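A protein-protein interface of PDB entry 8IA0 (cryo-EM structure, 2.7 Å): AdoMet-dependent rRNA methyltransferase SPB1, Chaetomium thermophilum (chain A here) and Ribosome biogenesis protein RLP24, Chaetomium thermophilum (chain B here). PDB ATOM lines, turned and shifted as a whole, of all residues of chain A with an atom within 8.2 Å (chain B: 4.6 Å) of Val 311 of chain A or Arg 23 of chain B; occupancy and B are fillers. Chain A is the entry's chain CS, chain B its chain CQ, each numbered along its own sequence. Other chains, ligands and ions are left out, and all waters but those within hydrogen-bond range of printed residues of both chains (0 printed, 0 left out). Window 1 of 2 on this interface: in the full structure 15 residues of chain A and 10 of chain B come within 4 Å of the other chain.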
ATOM      1  N   PRO A 235     -29.014 -14.322  20.977  1.00  0.00           N
ATOM      2  CA  PRO A 235     -28.563 -13.395  19.930  1.00  0.00           C
ATOM      3  C   PRO A 235     -28.688 -11.925  20.294  1.00  0.00           C
ATOM      4  O   PRO A 235     -28.227 -11.078  19.517  1.00  0.00           O
ATOM      5  CB  PRO A 235     -29.473 -13.744  18.748  1.00  0.00           C
ATOM      6  CG  PRO A 235     -30.725 -14.207  19.385  1.00  0.00           C
ATOM      7  CD  PRO A 235     -30.331 -14.901  20.663  1.00  0.00           C
ATOM      8  N   THR A 251     -16.495 -10.202   1.717  1.00  0.00           N
ATOM      9  CA  THR A 251     -17.863  -9.772   1.429  1.00  0.00           C
ATOM     10  C   THR A 251     -18.809 -10.146   2.566  1.00  0.00           C
ATOM     11  O   THR A 251     -19.976  -9.743   2.560  1.00  0.00           O
ATOM     12  CB  THR A 251     -18.378 -10.349   0.103  1.00  0.00           C
ATOM     13  OG1 THR A 251     -18.594 -11.759   0.236  1.00  0.00           O
ATOM     14  CG2 THR A 251     -17.382 -10.092  -1.020  1.00  0.00           C
ATOM     15  N   GLN A 252     -18.302 -10.895   3.547  1.00  0.00           N
ATOM     16  CA  GLN A 252     -19.012 -11.201   4.790  1.00  0.00           C
ATOM     17  C   GLN A 252     -20.438 -11.687   4.535  1.00  0.00           C
ATOM     18  O   GLN A 252     -21.384 -11.285   5.213  1.00  0.00           O
ATOM     19  CB  GLN A 252     -19.010  -9.989   5.723  1.00  0.00           C
ATOM     20  CG  GLN A 252     -17.625  -9.571   6.191  1.00  0.00           C
ATOM     21  CD  GLN A 252     -17.097 -10.435   7.316  1.00  0.00           C
ATOM     22  OE1 GLN A 252     -16.231 -11.283   7.107  1.00  0.00           O
ATOM     23  NE2 GLN A 252     -17.616 -10.224   8.518  1.00  0.00           N
ATOM     24  N   TYR A 253     -20.597 -12.567   3.549  1.00  0.00           N
ATOM     25  CA  TYR A 253     -21.911 -13.069   3.178  1.00  0.00           C
ATOM     26  C   TYR A 253     -21.812 -14.532   2.779  1.00  0.00           C
ATOM     27  O   TYR A 253     -20.877 -14.930   2.078  1.00  0.00           O
ATOM     28  CB  TYR A 253     -22.503 -12.250   2.029  1.00  0.00           C
ATOM     29  CG  TYR A 253     -23.983 -12.457   1.818  1.00  0.00           C
ATOM     30  CD1 TYR A 253     -24.907 -11.962   2.724  1.00  0.00           C
ATOM     31  CD2 TYR A 253     -24.455 -13.133   0.705  1.00  0.00           C
ATOM     32  CE1 TYR A 253     -26.261 -12.142   2.529  1.00  0.00           C
ATOM     33  CE2 TYR A 253     -25.806 -13.315   0.504  1.00  0.00           C
ATOM     34  CZ  TYR A 253     -26.704 -12.822   1.420  1.00  0.00           C
ATOM     35  OH  TYR A 253     -28.051 -13.005   1.222  1.00  0.00           O
ATOM     36  N   TYR A 274     -24.517 -18.312   8.977  1.00  0.00           N
ATOM     37  CA  TYR A 274     -24.965 -18.000   7.629  1.00  0.00           C
ATOM     38  C   TYR A 274     -25.979 -16.865   7.649  1.00  0.00           C
ATOM     39  O   TYR A 274     -26.585 -16.555   8.678  1.00  0.00           O
ATOM     40  CB  TYR A 274     -25.561 -19.234   6.942  1.00  0.00           C
ATOM     41  CG  TYR A 274     -24.504 -20.197   6.459  1.00  0.00           C
ATOM     42  CD1 TYR A 274     -23.831 -21.023   7.350  1.00  0.00           C
ATOM     43  CD2 TYR A 274     -24.173 -20.276   5.116  1.00  0.00           C
ATOM     44  CE1 TYR A 274     -22.859 -21.900   6.913  1.00  0.00           C
ATOM     45  CE2 TYR A 274     -23.199 -21.144   4.673  1.00  0.00           C
ATOM     46  CZ  TYR A 274     -22.549 -21.958   5.573  1.00  0.00           C
ATOM     47  OH  TYR A 274     -21.581 -22.831   5.132  1.00  0.00           O
ATOM     48  N   ASN A 275     -26.149 -16.242   6.486  1.00  0.00           N
ATOM     49  CA  ASN A 275     -26.984 -15.060   6.327  1.00  0.00           C
ATOM     50  C   ASN A 275     -28.357 -15.368   5.748  1.00  0.00           C
ATOM     51  O   ASN A 275     -29.333 -14.699   6.101  1.00  0.00           O
ATOM     52  CB  ASN A 275     -26.282 -14.042   5.422  1.00  0.00           C
ATOM     53  CG  ASN A 275     -25.122 -13.352   6.108  1.00  0.00           C
ATOM     54  OD1 ASN A 275     -23.962 -13.691   5.881  1.00  0.00           O
ATOM     55  ND2 ASN A 275     -25.429 -12.367   6.940  1.00  0.00           N
ATOM     56  N   LYS A 276     -28.459 -16.361   4.867  1.00  0.00           N
ATOM     57  CA  LYS A 276     -29.697 -16.618   4.142  1.00  0.00           C
ATOM     58  C   LYS A 276     -29.823 -18.100   3.827  1.00  0.00           C
ATOM     59  O   LYS A 276     -28.861 -18.722   3.366  1.00  0.00           O
ATOM     60  CB  LYS A 276     -29.745 -15.802   2.847  1.00  0.00           C
ATOM     61  CG  LYS A 276     -30.989 -16.032   2.010  1.00  0.00           C
ATOM     62  CD  LYS A 276     -31.024 -15.076   0.831  1.00  0.00           C
ATOM     63  CE  LYS A 276     -32.172 -15.389  -0.112  1.00  0.00           C
ATOM     64  NZ  LYS A 276     -33.492 -15.174   0.538  1.00  0.00           N
ATOM     65  N   ALA A 304     -39.867 -15.723   5.918  1.00  0.00           N
ATOM     66  CA  ALA A 304     -39.346 -14.431   6.355  1.00  0.00           C
ATOM     67  C   ALA A 304     -38.062 -14.590   7.161  1.00  0.00           C
ATOM     68  O   ALA A 304     -37.104 -13.831   6.974  1.00  0.00           O
ATOM     69  CB  ALA A 304     -40.402 -13.689   7.172  1.00  0.00           C
ATOM     70  N   CYS A 305     -38.025 -15.570   8.068  1.00  0.00           N
ATOM     71  CA  CYS A 305     -36.841 -15.770   8.896  1.00  0.00           C
ATOM     72  C   CYS A 305     -35.659 -16.257   8.070  1.00  0.00           C
ATOM     73  O   CYS A 305     -34.514 -15.857   8.313  1.00  0.00           O
ATOM     74  CB  CYS A 305     -37.149 -16.756  10.022  1.00  0.00           C
ATOM     75  SG  CYS A 305     -38.430 -16.213  11.171  1.00  0.00           S
ATOM     76  N   ASP A 307     -34.919 -15.590   5.049  1.00  0.00           N
ATOM     77  CA  ASP A 307     -34.366 -14.546   4.196  1.00  0.00           C
ATOM     78  C   ASP A 307     -33.302 -13.735   4.928  1.00  0.00           C
ATOM     79  O   ASP A 307     -32.293 -13.339   4.332  1.00  0.00           O
ATOM     80  CB  ASP A 307     -35.487 -13.636   3.695  1.00  0.00           C
ATOM     81  CG  ASP A 307     -35.289 -13.205   2.257  1.00  0.00           C
ATOM     82  OD1 ASP A 307     -34.452 -12.312   2.013  1.00  0.00           O
ATOM     83  OD2 ASP A 307     -35.971 -13.762   1.370  1.00  0.00           O
ATOM     84  N   ASP A 308     -33.509 -13.475   6.222  1.00  0.00           N
ATOM     85  CA  ASP A 308     -32.607 -12.651   7.031  1.00  0.00           C
ATOM     86  C   ASP A 308     -32.345 -13.390   8.342  1.00  0.00           C
ATOM     87  O   ASP A 308     -33.164 -13.359   9.263  1.00  0.00           O
ATOM     88  CB  ASP A 308     -33.204 -11.264   7.265  1.00  0.00           C
ATOM     89  CG  ASP A 308     -32.158 -10.167   7.247  1.00  0.00           C
ATOM     90  OD1 ASP A 308     -31.032 -10.408   7.728  1.00  0.00           O
ATOM     91  OD2 ASP A 308     -32.464  -9.063   6.751  1.00  0.00           O
ATOM     92  N   LEU A 309     -31.194 -14.061   8.419  1.00  0.00           N
ATOM     93  CA  LEU A 309     -30.871 -14.829   9.617  1.00  0.00           C
ATOM     94  C   LEU A 309     -30.228 -13.957  10.688  1.00  0.00           C
ATOM     95  O   LEU A 309     -30.289 -14.283  11.878  1.00  0.00           O
ATOM     96  CB  LEU A 309     -29.951 -15.996   9.263  1.00  0.00           C
ATOM     97  CG  LEU A 309     -30.593 -17.213   8.597  1.00  0.00           C
ATOM     98  CD1 LEU A 309     -29.533 -18.223   8.208  1.00  0.00           C
ATOM     99  CD2 LEU A 309     -31.626 -17.842   9.511  1.00  0.00           C
ATOM    100  N   LYS A 310     -29.605 -12.848  10.289  1.00  0.00           N
ATOM    101  CA  LYS A 310     -28.835 -12.046  11.231  1.00  0.00           C
ATOM    102  C   LYS A 310     -29.695 -11.098  12.058  1.00  0.00           C
ATOM    103  O   LYS A 310     -29.163 -10.432  12.951  1.00  0.00           O
ATOM    104  CB  LYS A 310     -27.765 -11.255  10.482  1.00  0.00           C
ATOM    105  CG  LYS A 310     -26.656 -12.118   9.917  1.00  0.00           C
ATOM    106  CD  LYS A 310     -25.810 -12.730  11.016  1.00  0.00           C
ATOM    107  CE  LYS A 310     -24.696 -13.582  10.438  1.00  0.00           C
ATOM    108  NZ  LYS A 310     -23.937 -14.299  11.498  1.00  0.00           N
ATOM    109  N   VAL A 311     -30.995 -11.021  11.789  1.00  0.00           N
ATOM    110  CA  VAL A 311     -31.901 -10.163  12.539  1.00  0.00           C
ATOM    111  C   VAL A 311     -32.860 -10.973  13.402  1.00  0.00           C
ATOM    112  O   VAL A 311     -33.797 -10.410  13.976  1.00  0.00           O
ATOM    113  CB  VAL A 311     -32.675  -9.220  11.605  1.00  0.00           C
ATOM    114  CG1 VAL A 311     -31.713  -8.391  10.777  1.00  0.00           C
ATOM    115  CG2 VAL A 311     -33.603 -10.014  10.708  1.00  0.00           C
ATOM    116  N   LEU A 312     -32.648 -12.280  13.514  1.00  0.00           N
ATOM    117  CA  LEU A 312     -33.576 -13.149  14.215  1.00  0.00           C
ATOM    118  C   LEU A 312     -33.326 -13.115  15.722  1.00  0.00           C
ATOM    119  O   LEU A 312     -32.289 -12.653  16.202  1.00  0.00           O
ATOM    120  CB  LEU A 312     -33.465 -14.578  13.690  1.00  0.00           C
ATOM    121  CG  LEU A 312     -33.949 -14.790  12.257  1.00  0.00           C
ATOM    122  CD1 LEU A 312     -34.035 -16.272  11.939  1.00  0.00           C
ATOM    123  CD2 LEU A 312     -35.289 -14.112  12.037  1.00  0.00           C
ATOM    124  N   GLY A 313     -34.303 -13.621  16.471  1.00  0.00           N
ATOM    125  CA  GLY A 313     -34.214 -13.682  17.916  1.00  0.00           C
ATOM    126  C   GLY A 313     -34.358 -15.088  18.461  1.00  0.00           C
ATOM    127  O   GLY A 313     -34.185 -16.065  17.727  1.00  0.00           O
ATOM    128  N   LYS A 314     -34.673 -15.203  19.754  1.00  0.00           N
ATOM    129  CA  LYS A 314     -34.783 -16.517  20.380  1.00  0.00           C
ATOM    130  C   LYS A 314     -35.965 -17.301  19.822  1.00  0.00           C
ATOM    131  O   LYS A 314     -35.824 -18.468  19.441  1.00  0.00           O
ATOM    132  CB  LYS A 314     -34.914 -16.366  21.895  1.00  0.00           C
ATOM    133  CG  LYS A 314     -33.598 -16.427  22.642  1.00  0.00           C
ATOM    134  CD  LYS A 314     -33.776 -16.527  24.158  1.00  0.00           C
ATOM    135  CE  LYS A 314     -34.974 -15.746  24.702  1.00  0.00           C
ATOM    136  NZ  LYS A 314     -35.084 -14.347  24.193  1.00  0.00           N
ATOM    137  N   ASP A 316     -37.638 -16.907  17.031  1.00  0.00           N
ATOM    138  CA  ASP A 316     -37.511 -17.207  15.608  1.00  0.00           C
ATOM    139  C   ASP A 316     -36.584 -18.391  15.370  1.00  0.00           C
ATOM    140  O   ASP A 316     -36.866 -19.246  14.523  1.00  0.00           O
ATOM    141  CB  ASP A 316     -37.018 -15.974  14.858  1.00  0.00           C
ATOM    142  CG  ASP A 316     -38.015 -14.835  14.893  1.00  0.00           C
ATOM    143  OD1 ASP A 316     -38.893 -14.844  15.780  1.00  0.00           O
ATOM    144  OD2 ASP A 316     -37.923 -13.934  14.034  1.00  0.00           O
ATOM    145  N   PHE A 317     -35.470 -18.456  16.101  1.00  0.00           N
ATOM    146  CA  PHE A 317     -34.533 -19.560  15.923  1.00  0.00           C
ATOM    147  C   PHE A 317     -35.141 -20.884  16.369  1.00  0.00           C
ATOM    148  O   PHE A 317     -34.950 -21.913  15.710  1.00  0.00           O
ATOM    149  CB  PHE A 317     -33.238 -19.272  16.680  1.00  0.00           C
ATOM    150  CG  PHE A 317     -32.255 -18.455  15.899  1.00  0.00           C
ATOM    151  CD1 PHE A 317     -32.073 -18.676  14.546  1.00  0.00           C
ATOM    152  CD2 PHE A 317     -31.513 -17.463  16.514  1.00  0.00           C
ATOM    153  CE1 PHE A 317     -31.169 -17.927  13.824  1.00  0.00           C
ATOM    154  CE2 PHE A 317     -30.608 -16.711  15.794  1.00  0.00           C
ATOM    155  CZ  PHE A 317     -30.436 -16.945  14.448  1.00  0.00           C
ATOM    156  N   PHE B  21     -28.232   2.104  10.099  1.00  0.00           N
ATOM    157  CA  PHE B  21     -27.291   1.073  10.518  1.00  0.00           C
ATOM    158  C   PHE B  21     -26.710   0.391   9.288  1.00  0.00           C
ATOM    159  O   PHE B  21     -27.455  -0.070   8.419  1.00  0.00           O
ATOM    160  CB  PHE B  21     -27.973   0.045  11.422  1.00  0.00           C
ATOM    161  CG  PHE B  21     -27.118  -1.145  11.742  1.00  0.00           C
ATOM    162  CD1 PHE B  21     -25.842  -0.984  12.248  1.00  0.00           C
ATOM    163  CD2 PHE B  21     -27.594  -2.428  11.540  1.00  0.00           C
ATOM    164  CE1 PHE B  21     -25.056  -2.079  12.545  1.00  0.00           C
ATOM    165  CE2 PHE B  21     -26.813  -3.527  11.836  1.00  0.00           C
ATOM    166  CZ  PHE B  21     -25.542  -3.351  12.339  1.00  0.00           C
ATOM    167  N   MET B  22     -25.385   0.328   9.222  1.00  0.00           N
ATOM    168  CA  MET B  22     -24.670  -0.275   8.106  1.00  0.00           C
ATOM    169  C   MET B  22     -24.110  -1.615   8.560  1.00  0.00           C
ATOM    170  O   MET B  22     -23.358  -1.676   9.539  1.00  0.00           O
ATOM    171  CB  MET B  22     -23.547   0.641   7.621  1.00  0.00           C
ATOM    172  CG  MET B  22     -23.915   1.508   6.433  1.00  0.00           C
ATOM    173  SD  MET B  22     -25.111   2.785   6.846  1.00  0.00           S
ATOM    174  CE  MET B  22     -25.436   3.477   5.228  1.00  0.00           C
ATOM    175  N   ARG B  23     -24.471  -2.681   7.855  1.00  0.00           N
ATOM    176  CA  ARG B  23     -24.054  -4.029   8.210  1.00  0.00           C
ATOM    177  C   ARG B  23     -22.905  -4.473   7.315  1.00  0.00           C
ATOM    178  O   ARG B  23     -22.800  -4.043   6.162  1.00  0.00           O
ATOM    179  CB  ARG B  23     -25.227  -5.006   8.103  1.00  0.00           C
ATOM    180  CG  ARG B  23     -25.269  -6.037   9.218  1.00  0.00           C
ATOM    181  CD  ARG B  23     -26.570  -6.824   9.221  1.00  0.00           C
ATOM    182  NE  ARG B  23     -26.824  -7.493   7.951  1.00  0.00           N
ATOM    183  CZ  ARG B  23     -27.921  -8.184   7.678  1.00  0.00           C
ATOM    184  NH1 ARG B  23     -28.890  -8.320   8.568  1.00  0.00           N
ATOM    185  NH2 ARG B  23     -28.051  -8.750   6.483  1.00  0.00           N
ATOM    186  N   ASN B  24     -22.037  -5.332   7.858  1.00  0.00           N
ATOM    187  CA  ASN B  24     -20.841  -5.754   7.135  1.00  0.00           C
ATOM    188  C   ASN B  24     -21.156  -6.537   5.869  1.00  0.00           C
ATOM    189  O   ASN B  24     -20.293  -6.641   4.991  1.00  0.00           O
ATOM    190  CB  ASN B  24     -19.939  -6.592   8.041  1.00  0.00           C
ATOM    191  CG  ASN B  24     -18.933  -5.754   8.795  1.00  0.00           C
ATOM    192  OD1 ASN B  24     -17.734  -6.024   8.761  1.00  0.00           O
ATOM    193  ND2 ASN B  24     -19.414  -4.722   9.473  1.00  0.00           N
ATOM    194  N   ASP B  25     -22.361  -7.094   5.747  1.00  0.00           N
ATOM    195  CA  ASP B  25     -22.715  -7.786   4.514  1.00  0.00           C
ATOM    196  C   ASP B  25     -22.978  -6.824   3.365  1.00  0.00           C
ATOM    197  O   ASP B  25     -23.078  -7.272   2.218  1.00  0.00           O
ATOM    198  CB  ASP B  25     -23.939  -8.677   4.736  1.00  0.00           C
ATOM    199  CG  ASP B  25     -25.221  -7.886   4.861  1.00  0.00           C
ATOM    200  OD1 ASP B  25     -25.478  -7.343   5.953  1.00  0.00           O
ATOM    201  OD2 ASP B  25     -25.972  -7.810   3.867  1.00  0.00           O
ATOM    202  N   GLY B  26     -23.085  -5.527   3.638  1.00  0.00           N
ATOM    203  CA  GLY B  26     -23.292  -4.547   2.592  1.00  0.00           C
ATOM    204  C   GLY B  26     -24.730  -4.094   2.472  1.00  0.00           C
ATOM    205  O   GLY B  26     -25.190  -3.741   1.382  1.00  0.00           O
ATOM    206  N   LYS B  27     -25.451  -4.098   3.588  1.00  0.00           N
ATOM    207  CA  LYS B  27     -26.852  -3.714   3.623  1.00  0.00           C
ATOM    208  C   LYS B  27     -27.048  -2.580   4.619  1.00  0.00           C
ATOM    209  O   LYS B  27     -26.432  -2.559   5.688  1.00  0.00           O
ATOM    210  CB  LYS B  27     -27.739  -4.905   4.000  1.00  0.00           C
ATOM    211  CG  LYS B  27     -29.227  -4.623   3.931  1.00  0.00           C
ATOM    212  CD  LYS B  27     -30.035  -5.880   4.195  1.00  0.00           C
ATOM    213  CE  LYS B  27     -31.521  -5.573   4.273  1.00  0.00           C
ATOM    214  NZ  LYS B  27     -32.063  -5.121   2.962  1.00  0.00           N
ATOM    215  N   PHE B  29     -29.800  -0.339   6.891  1.00  0.00           N
ATOM    216  CA  PHE B  29     -31.108  -0.324   7.527  1.00  0.00           C
ATOM    217  C   PHE B  29     -31.429   1.096   7.969  1.00  0.00           C
ATOM    218  O   PHE B  29     -30.620   1.732   8.650  1.00  0.00           O
ATOM    219  CB  PHE B  29     -31.148  -1.266   8.732  1.00  0.00           C
ATOM    220  CG  PHE B  29     -30.859  -2.699   8.397  1.00  0.00           C
ATOM    221  CD1 PHE B  29     -29.560  -3.176   8.403  1.00  0.00           C
ATOM    222  CD2 PHE B  29     -31.885  -3.574   8.097  1.00  0.00           C
ATOM    223  CE1 PHE B  29     -29.292  -4.495   8.104  1.00  0.00           C
ATOM    224  CE2 PHE B  29     -31.622  -4.892   7.797  1.00  0.00           C
ATOM    225  CZ  PHE B  29     -30.324  -5.352   7.800  1.00  0.00           C
ATOM    226  N   PHE B  40     -35.035  -3.023  17.032  1.00  0.00           N
ATOM    227  CA  PHE B  40     -34.212  -3.781  16.097  1.00  0.00           C
ATOM    228  C   PHE B  40     -32.985  -4.373  16.783  1.00  0.00           C
ATOM    229  O   PHE B  40     -32.611  -5.521  16.516  1.00  0.00           O
ATOM    230  CB  PHE B  40     -33.800  -2.887  14.929  1.00  0.00           C
ATOM    231  CG  PHE B  40     -33.031  -3.599  13.859  1.00  0.00           C
ATOM    232  CD1 PHE B  40     -33.689  -4.314  12.878  1.00  0.00           C
ATOM    233  CD2 PHE B  40     -31.651  -3.536  13.822  1.00  0.00           C
ATOM    234  CE1 PHE B  40     -32.983  -4.964  11.889  1.00  0.00           C
ATOM    235  CE2 PHE B  40     -30.942  -4.182  12.835  1.00  0.00           C
ATOM    236  CZ  PHE B  40     -31.609  -4.897  11.869  1.00  0.00           C
ATOM    237  N   LYS B  43     -33.623  -7.484  18.691  1.00  0.00           N
ATOM    238  CA  LYS B  43     -33.981  -8.623  17.850  1.00  0.00           C
ATOM    239  C   LYS B  43     -35.455  -8.994  17.969  1.00  0.00           C
ATOM    240  O   LYS B  43     -35.812 -10.170  17.876  1.00  0.00           O
ATOM    241  CB  LYS B  43     -33.099  -9.837  18.151  1.00  0.00           C
ATOM    242  CG  LYS B  43     -31.611  -9.555  18.050  1.00  0.00           C
ATOM    243  CD  LYS B  43     -31.191  -9.312  16.615  1.00  0.00           C
ATOM    244  CE  LYS B  43     -29.793  -9.835  16.356  1.00  0.00           C
ATOM    245  NZ  LYS B  43     -28.791  -9.182  17.236  1.00  0.00           N
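Hydrophobic or aromatic side chains of chain B within 4 Å of the printed part of chain A: Phe 40.
The guanidinium group (NE) of Arg 23 of chain B lies within salt-bridge range of the side-chain carboxylate (OD1) of Asp 25 of chain B (2.4 Å).
Asn 24 of chain B touches Thr 251 of chain A. Thr 251 of chain A touches Asp 25 of chain B (O to CA, 3.9 Å). O of Asn 24 of chain B touches CB of Gln 252 of chain A (3.7 Å). Gln 252 of chain A touches Asp 25 of chain B (O to CB, 3.7 Å). Tyr 253 of chain A touches Asp 25 of chain B (CD1 to CB, 3.97 Å). Lys 310 of chain A touches Arg 23 of chain B (CB to NH1, 3.7 Å). CG1 of Val 311 of chain A touches NH1 of Arg 23 of chain B, 3.6 Å away. CG1 of Val 311 of chain A touches CZ of Phe 40 of chain B (3.7 Å). O of Val 311 of chain A touches CD of Lys 43 of chain B (3.9 Å). CA of Gly 313 of chain A touches O of Lys 43 of chain B (3.9 Å).
The side-chain carboxylate (OD1) of Asp 308 of chain A lies within salt-bridge range of the guanidinium group (NH1) of Arg 23 of chain B, at 3.1 Å. The backbone carbonyl oxygen (O) of Pro 235 of chain A sits at hydrogen-bond distance from the side-chain amino group (NZ) of Lys 43 of chain B, 3.0 Å away.
Of chain B, only Arg 23 (3.6 Å), Phe 40 (3.7 Å) and Lys 43 (3.9 Å) come within 4 Å of Val 311 of chain A. Printed residues of chain A within 4 Å of Arg 23 of chain B: Asp 308 (3.1 Å), Lys 310 (3.7 Å) and Val 311 (3.6 Å). Printed residues of chain B within 4 Å of Asp 308 of chain A: Arg 23. Printed residues of chain B within 4 Å of Tyr 253 of chain A: Asp 25. Of the printed residues of chain B, Leu 312 of chain A touches Lys 43. Of the printed residues of chain A, Asn 24 of chain B touches Thr 251 and Gln 252. Of the printed residues of chain A, Lys 43 of chain B touches Pro 235, Lys 310, Val 311, Leu 312 and Gly 313. Asn 275 of chain A touches none of the printed residues of chain B. The nearest printed residue of chain A that does not touch Asn 24 of chain B is Tyr 253 of chain A (6.1 Å).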
